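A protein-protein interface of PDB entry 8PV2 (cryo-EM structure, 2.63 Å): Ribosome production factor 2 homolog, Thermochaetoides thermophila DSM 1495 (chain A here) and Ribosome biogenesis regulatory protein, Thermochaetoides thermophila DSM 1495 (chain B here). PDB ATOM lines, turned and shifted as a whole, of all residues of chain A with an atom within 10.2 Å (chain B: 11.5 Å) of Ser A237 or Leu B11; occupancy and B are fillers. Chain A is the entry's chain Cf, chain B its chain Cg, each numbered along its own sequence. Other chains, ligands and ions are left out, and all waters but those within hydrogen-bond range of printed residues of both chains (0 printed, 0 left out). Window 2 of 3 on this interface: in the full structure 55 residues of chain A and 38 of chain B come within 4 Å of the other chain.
Printed residues of chain A that touch a printed residue of chain B: Ser A237, Thr A239, Leu A241, Pro A242, Arg A243, Val A244 and Glu A245. Hydrophobic or aromatic side chains of chain A within 4 Å of the printed part of chain B: Leu A241, Pro A242 and Val A244. Hydrophobic or aromatic side chains of chain B within 4 Å of the printed part of chain A: Leu B11, Val B13 and Leu B67. Along chain B the printed residues that touch a printed residue of chain A span positions 11 to 68. Among the printed residues, 17 pairs touch across the chains.
Ser A237 touches just these residues of chain B: Leu B11 (3.8 Å) and Val B13 (3.4 Å). No residue of chain B comes within 4 Å of Gly A238. Of chain B, only Leu B11 (3.9 Å), Pro B12 (2.7 Å), Val B13 (3.9 Å), Arg B56 (3.8 Å) and Gln B60 (3.8 Å) come within 4 Å of Arg A243. Of the printed residues of chain B, Val A244 touches Arg B56 (3.1 Å) and Gln B60 (2.9 Å). Leu B11 touches two residues of chain A. Of the printed residues of chain A, Val B13 touches Ser A237 (3.4 Å), Thr A239 (3.8 Å), Leu A241 (3.7 Å), Pro A242 (3.4 Å) and Arg A243 (3.9 Å). Of the printed residues of chain A, Arg B56 touches Arg A243 (3.8 Å), Val A244 (3.1 Å) and Glu A245 (3.9 Å). The nearest residue of chain B that does not touch Ser A237 is Pro B12 (5.6 Å).
ND2 of Asn B64 is in hydrogen-bond range of O of Val B13 (2.7 Å). NE2 of Gln B60 lies within hydrogen-bond range of OD1 of Asn B64 (3.0 Å). The side-chain hydroxyl (OG1) of Thr B68 is in hydrogen-bond range of the backbone carbonyl oxygen (O) of Asn B64, at 2.5 Å. O of Lys A235 lies within hydrogen-bond range of N of Arg A243. NE of Arg A243 is in salt-bridge range of OE2 of Glu A245 (2.6 Å). The guanidinium group (NH1) of Arg B56 sits at hydrogen-bond distance from the side-chain amide oxygen (OE1) of Gln B60.
The backbone NH (N) of Val A244 sits at hydrogen-bond distance from the side-chain amide oxygen (OE1) of Gln B60, 2.9 Å away. The guanidinium group (NH1) of Arg B56 is in hydrogen-bond range of the backbone carbonyl oxygen (O) of Val A244, 3.1 Å away. The backbone carbonyl oxygen (O) of Pro B12 lies within hydrogen-bond range of the guanidinium group (NH1) of Arg A243. The backbone carbonyl oxygen of Pro A242 is in hydrogen-bond range of the side-chain amide nitrogen of Gln B60.
Among the printed residues, pairs that only touch across the chains: Pro A242 with Val B13, Ser A237 with Val B13, Leu A241 with Asn B64, Leu A241 with Val B13, Pro A242 with Leu B67, Arg A243 with Arg B56, Ser A237 with Leu B11, Arg A243 with Gln B60, Thr A239 with Val B13, Glu A245 with Arg B56, Arg A243 with Val B13, Arg A243 with Leu B11 and Leu A241 with Thr B68.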
ATOM      1  N   THR A 234      24.440  -2.054 -29.693  1.00  0.00           N
ATOM      2  CA  THR A 234      23.895  -2.149 -28.347  1.00  0.00           C
ATOM      3  C   THR A 234      23.509  -3.589 -28.039  1.00  0.00           C
ATOM      4  O   THR A 234      23.019  -4.309 -28.912  1.00  0.00           O
ATOM      5  CB  THR A 234      22.675  -1.238 -28.178  1.00  0.00           C
ATOM      6  OG1 THR A 234      21.671  -1.603 -29.131  1.00  0.00           O
ATOM      7  CG2 THR A 234      23.061   0.214 -28.395  1.00  0.00           C
ATOM      8  N   LYS A 235      23.728  -4.001 -26.791  1.00  0.00           N
ATOM      9  CA  LYS A 235      23.490  -5.369 -26.355  1.00  0.00           C
ATOM     10  C   LYS A 235      22.704  -5.371 -25.050  1.00  0.00           C
ATOM     11  O   LYS A 235      22.689  -4.384 -24.311  1.00  0.00           O
ATOM     12  CB  LYS A 235      24.806  -6.130 -26.164  1.00  0.00           C
ATOM     13  CG  LYS A 235      25.581  -6.356 -27.442  1.00  0.00           C
ATOM     14  CD  LYS A 235      26.837  -7.157 -27.182  1.00  0.00           C
ATOM     15  CE  LYS A 235      27.653  -7.319 -28.451  1.00  0.00           C
ATOM     16  NZ  LYS A 235      26.957  -8.177 -29.447  1.00  0.00           N
ATOM     17  N   ARG A 236      22.041  -6.495 -24.776  1.00  0.00           N
ATOM     18  CA  ARG A 236      21.311  -6.648 -23.522  1.00  0.00           C
ATOM     19  C   ARG A 236      22.282  -6.765 -22.356  1.00  0.00           C
ATOM     20  O   ARG A 236      23.351  -7.368 -22.481  1.00  0.00           O
ATOM     21  CB  ARG A 236      20.399  -7.875 -23.563  1.00  0.00           C
ATOM     22  CG  ARG A 236      19.395  -7.840 -24.682  1.00  0.00           C
ATOM     23  CD  ARG A 236      18.402  -8.973 -24.662  1.00  0.00           C
ATOM     24  NE  ARG A 236      17.461  -8.831 -25.766  1.00  0.00           N
ATOM     25  CZ  ARG A 236      16.337  -8.131 -25.708  1.00  0.00           C
ATOM     26  NH1 ARG A 236      15.972  -7.498 -24.606  1.00  0.00           N
ATOM     27  NH2 ARG A 236      15.561  -8.059 -26.786  1.00  0.00           N
ATOM     28  N   SER A 237      21.906  -6.184 -21.218  1.00  0.00           N
ATOM     29  CA  SER A 237      22.724  -6.234 -20.014  1.00  0.00           C
ATOM     30  C   SER A 237      21.930  -6.653 -18.786  1.00  0.00           C
ATOM     31  O   SER A 237      22.480  -6.663 -17.680  1.00  0.00           O
ATOM     32  CB  SER A 237      23.382  -4.876 -19.766  1.00  0.00           C
ATOM     33  OG  SER A 237      22.424  -3.920 -19.350  1.00  0.00           O
ATOM     34  N   GLY A 238      20.656  -6.995 -18.946  1.00  0.00           N
ATOM     35  CA  GLY A 238      19.809  -7.292 -17.813  1.00  0.00           C
ATOM     36  C   GLY A 238      19.244  -6.080 -17.113  1.00  0.00           C
ATOM     37  O   GLY A 238      18.481  -6.239 -16.153  1.00  0.00           O
ATOM     38  N   THR A 239      19.591  -4.875 -17.558  1.00  0.00           N
ATOM     39  CA  THR A 239      19.079  -3.632 -17.007  1.00  0.00           C
ATOM     40  C   THR A 239      18.320  -2.891 -18.098  1.00  0.00           C
ATOM     41  O   THR A 239      18.212  -3.357 -19.237  1.00  0.00           O
ATOM     42  CB  THR A 239      20.209  -2.754 -16.455  1.00  0.00           C
ATOM     43  OG1 THR A 239      20.899  -2.128 -17.544  1.00  0.00           O
ATOM     44  CG2 THR A 239      21.196  -3.583 -15.650  1.00  0.00           C
ATOM     45  N   ARG A 240      17.784  -1.724 -17.739  1.00  0.00           N
ATOM     46  CA  ARG A 240      17.098  -0.889 -18.720  1.00  0.00           C
ATOM     47  C   ARG A 240      18.076  -0.330 -19.745  1.00  0.00           C
ATOM     48  O   ARG A 240      17.767  -0.248 -20.939  1.00  0.00           O
ATOM     49  CB  ARG A 240      16.354   0.242 -18.010  1.00  0.00           C
ATOM     50  CG  ARG A 240      15.236   0.880 -18.822  1.00  0.00           C
ATOM     51  CD  ARG A 240      14.385  -0.157 -19.540  1.00  0.00           C
ATOM     52  NE  ARG A 240      13.102   0.395 -19.961  1.00  0.00           N
ATOM     53  CZ  ARG A 240      12.428  -0.005 -21.032  1.00  0.00           C
ATOM     54  NH1 ARG A 240      12.885  -0.964 -21.819  1.00  0.00           N
ATOM     55  NH2 ARG A 240      11.265   0.573 -21.318  1.00  0.00           N
ATOM     56  N   LEU A 241      19.262   0.064 -19.296  1.00  0.00           N
ATOM     57  CA  LEU A 241      20.237   0.659 -20.193  1.00  0.00           C
ATOM     58  C   LEU A 241      20.939  -0.423 -21.008  1.00  0.00           C
ATOM     59  O   LEU A 241      21.257  -1.492 -20.479  1.00  0.00           O
ATOM     60  CB  LEU A 241      21.260   1.462 -19.395  1.00  0.00           C
ATOM     61  CG  LEU A 241      20.674   2.657 -18.646  1.00  0.00           C
ATOM     62  CD1 LEU A 241      21.741   3.341 -17.813  1.00  0.00           C
ATOM     63  CD2 LEU A 241      20.024   3.631 -19.611  1.00  0.00           C
ATOM     64  N   PRO A 242      21.189  -0.183 -22.292  1.00  0.00           N
ATOM     65  CA  PRO A 242      21.909  -1.166 -23.104  1.00  0.00           C
ATOM     66  C   PRO A 242      23.409  -1.116 -22.865  1.00  0.00           C
ATOM     67  O   PRO A 242      23.962  -0.134 -22.369  1.00  0.00           O
ATOM     68  CB  PRO A 242      21.573  -0.742 -24.536  1.00  0.00           C
ATOM     69  CG  PRO A 242      21.386   0.719 -24.434  1.00  0.00           C
ATOM     70  CD  PRO A 242      20.768   0.981 -23.087  1.00  0.00           C
ATOM     71  N   ARG A 243      24.067  -2.208 -23.240  1.00  0.00           N
ATOM     72  CA  ARG A 243      25.520  -2.291 -23.199  1.00  0.00           C
ATOM     73  C   ARG A 243      26.072  -1.861 -24.551  1.00  0.00           C
ATOM     74  O   ARG A 243      25.748  -2.464 -25.580  1.00  0.00           O
ATOM     75  CB  ARG A 243      25.975  -3.707 -22.850  1.00  0.00           C
ATOM     76  CG  ARG A 243      27.429  -3.988 -23.181  1.00  0.00           C
ATOM     77  CD  ARG A 243      28.359  -3.371 -22.157  1.00  0.00           C
ATOM     78  NE  ARG A 243      29.760  -3.613 -22.474  1.00  0.00           N
ATOM     79  CZ  ARG A 243      30.767  -3.311 -21.669  1.00  0.00           C
ATOM     80  NH1 ARG A 243      30.564  -2.762 -20.484  1.00  0.00           N
ATOM     81  NH2 ARG A 243      32.012  -3.564 -22.062  1.00  0.00           N
ATOM     82  N   VAL A 244      26.896  -0.823 -24.548  1.00  0.00           N
ATOM     83  CA  VAL A 244      27.416  -0.245 -25.779  1.00  0.00           C
ATOM     84  C   VAL A 244      28.736  -0.910 -26.134  1.00  0.00           C
ATOM     85  O   VAL A 244      29.632  -1.036 -25.294  1.00  0.00           O
ATOM     86  CB  VAL A 244      27.579   1.276 -25.625  1.00  0.00           C
ATOM     87  CG1 VAL A 244      28.254   1.872 -26.843  1.00  0.00           C
ATOM     88  CG2 VAL A 244      26.230   1.923 -25.383  1.00  0.00           C
ATOM     89  N   GLU A 245      28.854  -1.351 -27.384  1.00  0.00           N
ATOM     90  CA  GLU A 245      30.102  -1.863 -27.920  1.00  0.00           C
ATOM     91  C   GLU A 245      30.401  -1.115 -29.209  1.00  0.00           C
ATOM     92  O   GLU A 245      29.494  -0.812 -29.985  1.00  0.00           O
ATOM     93  CB  GLU A 245      30.025  -3.373 -28.182  1.00  0.00           C
ATOM     94  CG  GLU A 245      29.718  -4.210 -26.945  1.00  0.00           C
ATOM     95  CD  GLU A 245      30.865  -4.263 -25.950  1.00  0.00           C
ATOM     96  OE1 GLU A 245      32.026  -4.036 -26.353  1.00  0.00           O
ATOM     97  OE2 GLU A 245      30.600  -4.519 -24.757  1.00  0.00           O
ATOM     98  N   LEU B  11      27.737  -7.812 -18.412  1.00  0.00           N
ATOM     99  CA  LEU B  11      28.681  -6.703 -18.459  1.00  0.00           C
ATOM    100  C   LEU B  11      28.020  -5.420 -17.961  1.00  0.00           C
ATOM    101  O   LEU B  11      26.846  -5.183 -18.233  1.00  0.00           O
ATOM    102  CB  LEU B  11      29.220  -6.523 -19.879  1.00  0.00           C
ATOM    103  CG  LEU B  11      30.432  -7.392 -20.221  1.00  0.00           C
ATOM    104  CD1 LEU B  11      30.574  -7.564 -21.724  1.00  0.00           C
ATOM    105  CD2 LEU B  11      31.700  -6.808 -19.621  1.00  0.00           C
ATOM    106  N   PRO B  12      28.769  -4.605 -17.220  1.00  0.00           N
ATOM    107  CA  PRO B  12      28.181  -3.399 -16.632  1.00  0.00           C
ATOM    108  C   PRO B  12      27.895  -2.329 -17.672  1.00  0.00           C
ATOM    109  O   PRO B  12      28.496  -2.293 -18.748  1.00  0.00           O
ATOM    110  CB  PRO B  12      29.253  -2.934 -15.642  1.00  0.00           C
ATOM    111  CG  PRO B  12      30.523  -3.430 -16.233  1.00  0.00           C
ATOM    112  CD  PRO B  12      30.188  -4.758 -16.850  1.00  0.00           C
ATOM    113  N   VAL B  13      26.955  -1.450 -17.336  1.00  0.00           N
ATOM    114  CA  VAL B  13      26.605  -0.317 -18.178  1.00  0.00           C
ATOM    115  C   VAL B  13      27.007   1.003 -17.524  1.00  0.00           C
ATOM    116  O   VAL B  13      26.625   2.070 -17.998  1.00  0.00           O
ATOM    117  CB  VAL B  13      25.112  -0.322 -18.535  1.00  0.00           C
ATOM    118  CG1 VAL B  13      24.790  -1.502 -19.419  1.00  0.00           C
ATOM    119  CG2 VAL B  13      24.266  -0.342 -17.275  1.00  0.00           C
ATOM    120  N   THR B  14      27.770   0.948 -16.440  1.00  0.00           N
ATOM    121  CA  THR B  14      28.236   2.144 -15.760  1.00  0.00           C
ATOM    122  C   THR B  14      29.735   2.037 -15.534  1.00  0.00           C
ATOM    123  O   THR B  14      30.236   1.003 -15.085  1.00  0.00           O
ATOM    124  CB  THR B  14      27.524   2.346 -14.418  1.00  0.00           C
ATOM    125  OG1 THR B  14      26.120   2.115 -14.584  1.00  0.00           O
ATOM    126  CG2 THR B  14      27.734   3.764 -13.913  1.00  0.00           C
ATOM    127  N   VAL B  15      30.448   3.113 -15.849  1.00  0.00           N
ATOM    128  CA  VAL B  15      31.894   3.167 -15.685  1.00  0.00           C
ATOM    129  C   VAL B  15      32.216   4.147 -14.569  1.00  0.00           C
ATOM    130  O   VAL B  15      31.409   5.025 -14.245  1.00  0.00           O
ATOM    131  CB  VAL B  15      32.610   3.566 -16.991  1.00  0.00           C
ATOM    132  CG1 VAL B  15      32.271   2.579 -18.097  1.00  0.00           C
ATOM    133  CG2 VAL B  15      32.239   4.972 -17.397  1.00  0.00           C
ATOM    134  N   GLN B  49      43.194  -0.800 -29.351  1.00  0.00           N
ATOM    135  CA  GLN B  49      42.320  -1.396 -28.345  1.00  0.00           C
ATOM    136  C   GLN B  49      42.088  -0.441 -27.180  1.00  0.00           C
ATOM    137  O   GLN B  49      40.958  -0.307 -26.692  1.00  0.00           O
ATOM    138  CB  GLN B  49      42.915  -2.716 -27.857  1.00  0.00           C
ATOM    139  CG  GLN B  49      41.899  -3.704 -27.305  1.00  0.00           C
ATOM    140  CD  GLN B  49      41.501  -3.407 -25.872  1.00  0.00           C
ATOM    141  OE1 GLN B  49      42.263  -2.804 -25.115  1.00  0.00           O
ATOM    142  NE2 GLN B  49      40.300  -3.826 -25.493  1.00  0.00           N
ATOM    143  N   SER B  53      38.576   1.328 -26.160  1.00  0.00           N
ATOM    144  CA  SER B  53      37.988   1.286 -24.823  1.00  0.00           C
ATOM    145  C   SER B  53      37.582   2.679 -24.351  1.00  0.00           C
ATOM    146  O   SER B  53      36.519   2.848 -23.736  1.00  0.00           O
ATOM    147  CB  SER B  53      38.962   0.659 -23.834  1.00  0.00           C
ATOM    148  OG  SER B  53      40.208   1.322 -23.876  1.00  0.00           O
ATOM    149  N   ARG B  56      34.464   3.524 -26.242  1.00  0.00           N
ATOM    150  CA  ARG B  56      33.342   2.755 -25.722  1.00  0.00           C
ATOM    151  C   ARG B  56      32.813   3.361 -24.433  1.00  0.00           C
ATOM    152  O   ARG B  56      31.597   3.450 -24.238  1.00  0.00           O
ATOM    153  CB  ARG B  56      33.777   1.308 -25.500  1.00  0.00           C
ATOM    154  CG  ARG B  56      32.669   0.280 -25.591  1.00  0.00           C
ATOM    155  CD  ARG B  56      32.753  -0.725 -24.457  1.00  0.00           C
ATOM    156  NE  ARG B  56      32.951  -0.092 -23.160  1.00  0.00           N
ATOM    157  CZ  ARG B  56      31.982   0.452 -22.438  1.00  0.00           C
ATOM    158  NH1 ARG B  56      30.724   0.428 -22.840  1.00  0.00           N
ATOM    159  NH2 ARG B  56      32.282   1.024 -21.277  1.00  0.00           N
ATOM    160  N   ASP B  57      33.714   3.793 -23.546  1.00  0.00           N
ATOM    161  CA  ASP B  57      33.288   4.415 -22.295  1.00  0.00           C
ATOM    162  C   ASP B  57      32.545   5.723 -22.548  1.00  0.00           C
ATOM    163  O   ASP B  57      31.495   5.985 -21.940  1.00  0.00           O
ATOM    164  CB  ASP B  57      34.499   4.650 -21.395  1.00  0.00           C
ATOM    165  CG  ASP B  57      35.098   3.359 -20.877  1.00  0.00           C
ATOM    166  OD1 ASP B  57      34.349   2.374 -20.721  1.00  0.00           O
ATOM    167  OD2 ASP B  57      36.321   3.328 -20.626  1.00  0.00           O
ATOM    168  N   GLN B  60      29.150   4.957 -24.032  1.00  0.00           N
ATOM    169  CA  GLN B  60      28.269   4.392 -23.018  1.00  0.00           C
ATOM    170  C   GLN B  60      27.683   5.473 -22.123  1.00  0.00           C
ATOM    171  O   GLN B  60      26.471   5.493 -21.876  1.00  0.00           O
ATOM    172  CB  GLN B  60      29.028   3.364 -22.183  1.00  0.00           C
ATOM    173  CG  GLN B  60      28.206   2.747 -21.077  1.00  0.00           C
ATOM    174  CD  GLN B  60      27.223   1.729 -21.590  1.00  0.00           C
ATOM    175  OE1 GLN B  60      27.605   0.748 -22.223  1.00  0.00           O
ATOM    176  NE2 GLN B  60      25.946   1.956 -21.326  1.00  0.00           N
ATOM    177  N   ILE B  63      25.148   7.567 -24.115  1.00  0.00           N
ATOM    178  CA  ILE B  63      23.883   6.870 -24.339  1.00  0.00           C
ATOM    179  C   ILE B  63      23.065   6.826 -23.054  1.00  0.00           C
ATOM    180  O   ILE B  63      21.846   7.038 -23.068  1.00  0.00           O
ATOM    181  CB  ILE B  63      24.145   5.462 -24.907  1.00  0.00           C
ATOM    182  CG1 ILE B  63      24.601   5.553 -26.364  1.00  0.00           C
ATOM    183  CG2 ILE B  63      22.911   4.584 -24.814  1.00  0.00           C
ATOM    184  CD1 ILE B  63      23.622   6.249 -27.270  1.00  0.00           C
ATOM    185  N   ASN B  64      23.730   6.574 -21.919  1.00  0.00           N
ATOM    186  CA  ASN B  64      23.031   6.563 -20.637  1.00  0.00           C
ATOM    187  C   ASN B  64      22.449   7.930 -20.304  1.00  0.00           C
ATOM    188  O   ASN B  64      21.301   8.028 -19.855  1.00  0.00           O
ATOM    189  CB  ASN B  64      23.974   6.105 -19.529  1.00  0.00           C
ATOM    190  CG  ASN B  64      24.435   4.679 -19.710  1.00  0.00           C
ATOM    191  OD1 ASN B  64      23.833   3.911 -20.454  1.00  0.00           O
ATOM    192  ND2 ASN B  64      25.509   4.315 -19.021  1.00  0.00           N
ATOM    193  N   LEU B  67      19.434   8.604 -22.616  1.00  0.00           N
ATOM    194  CA  LEU B  67      18.280   7.769 -22.323  1.00  0.00           C
ATOM    195  C   LEU B  67      17.702   7.997 -20.935  1.00  0.00           C
ATOM    196  O   LEU B  67      16.576   7.562 -20.680  1.00  0.00           O
ATOM    197  CB  LEU B  67      18.647   6.293 -22.476  1.00  0.00           C
ATOM    198  CG  LEU B  67      18.882   5.776 -23.892  1.00  0.00           C
ATOM    199  CD1 LEU B  67      19.186   4.292 -23.862  1.00  0.00           C
ATOM    200  CD2 LEU B  67      17.684   6.061 -24.778  1.00  0.00           C
ATOM    201  N   THR B  68      18.431   8.653 -20.031  1.00  0.00           N
ATOM    202  CA  THR B  68      17.920   8.874 -18.688  1.00  0.00           C
ATOM    203  C   THR B  68      17.480  10.299 -18.389  1.00  0.00           C
ATOM    204  O   THR B  68      16.546  10.472 -17.599  1.00  0.00           O
ATOM    205  CB  THR B  68      18.962   8.459 -17.639  1.00  0.00           C
ATOM    206  OG1 THR B  68      20.204   9.118 -17.908  1.00  0.00           O
ATOM    207  CG2 THR B  68      19.162   6.955 -17.652  1.00  0.00           C
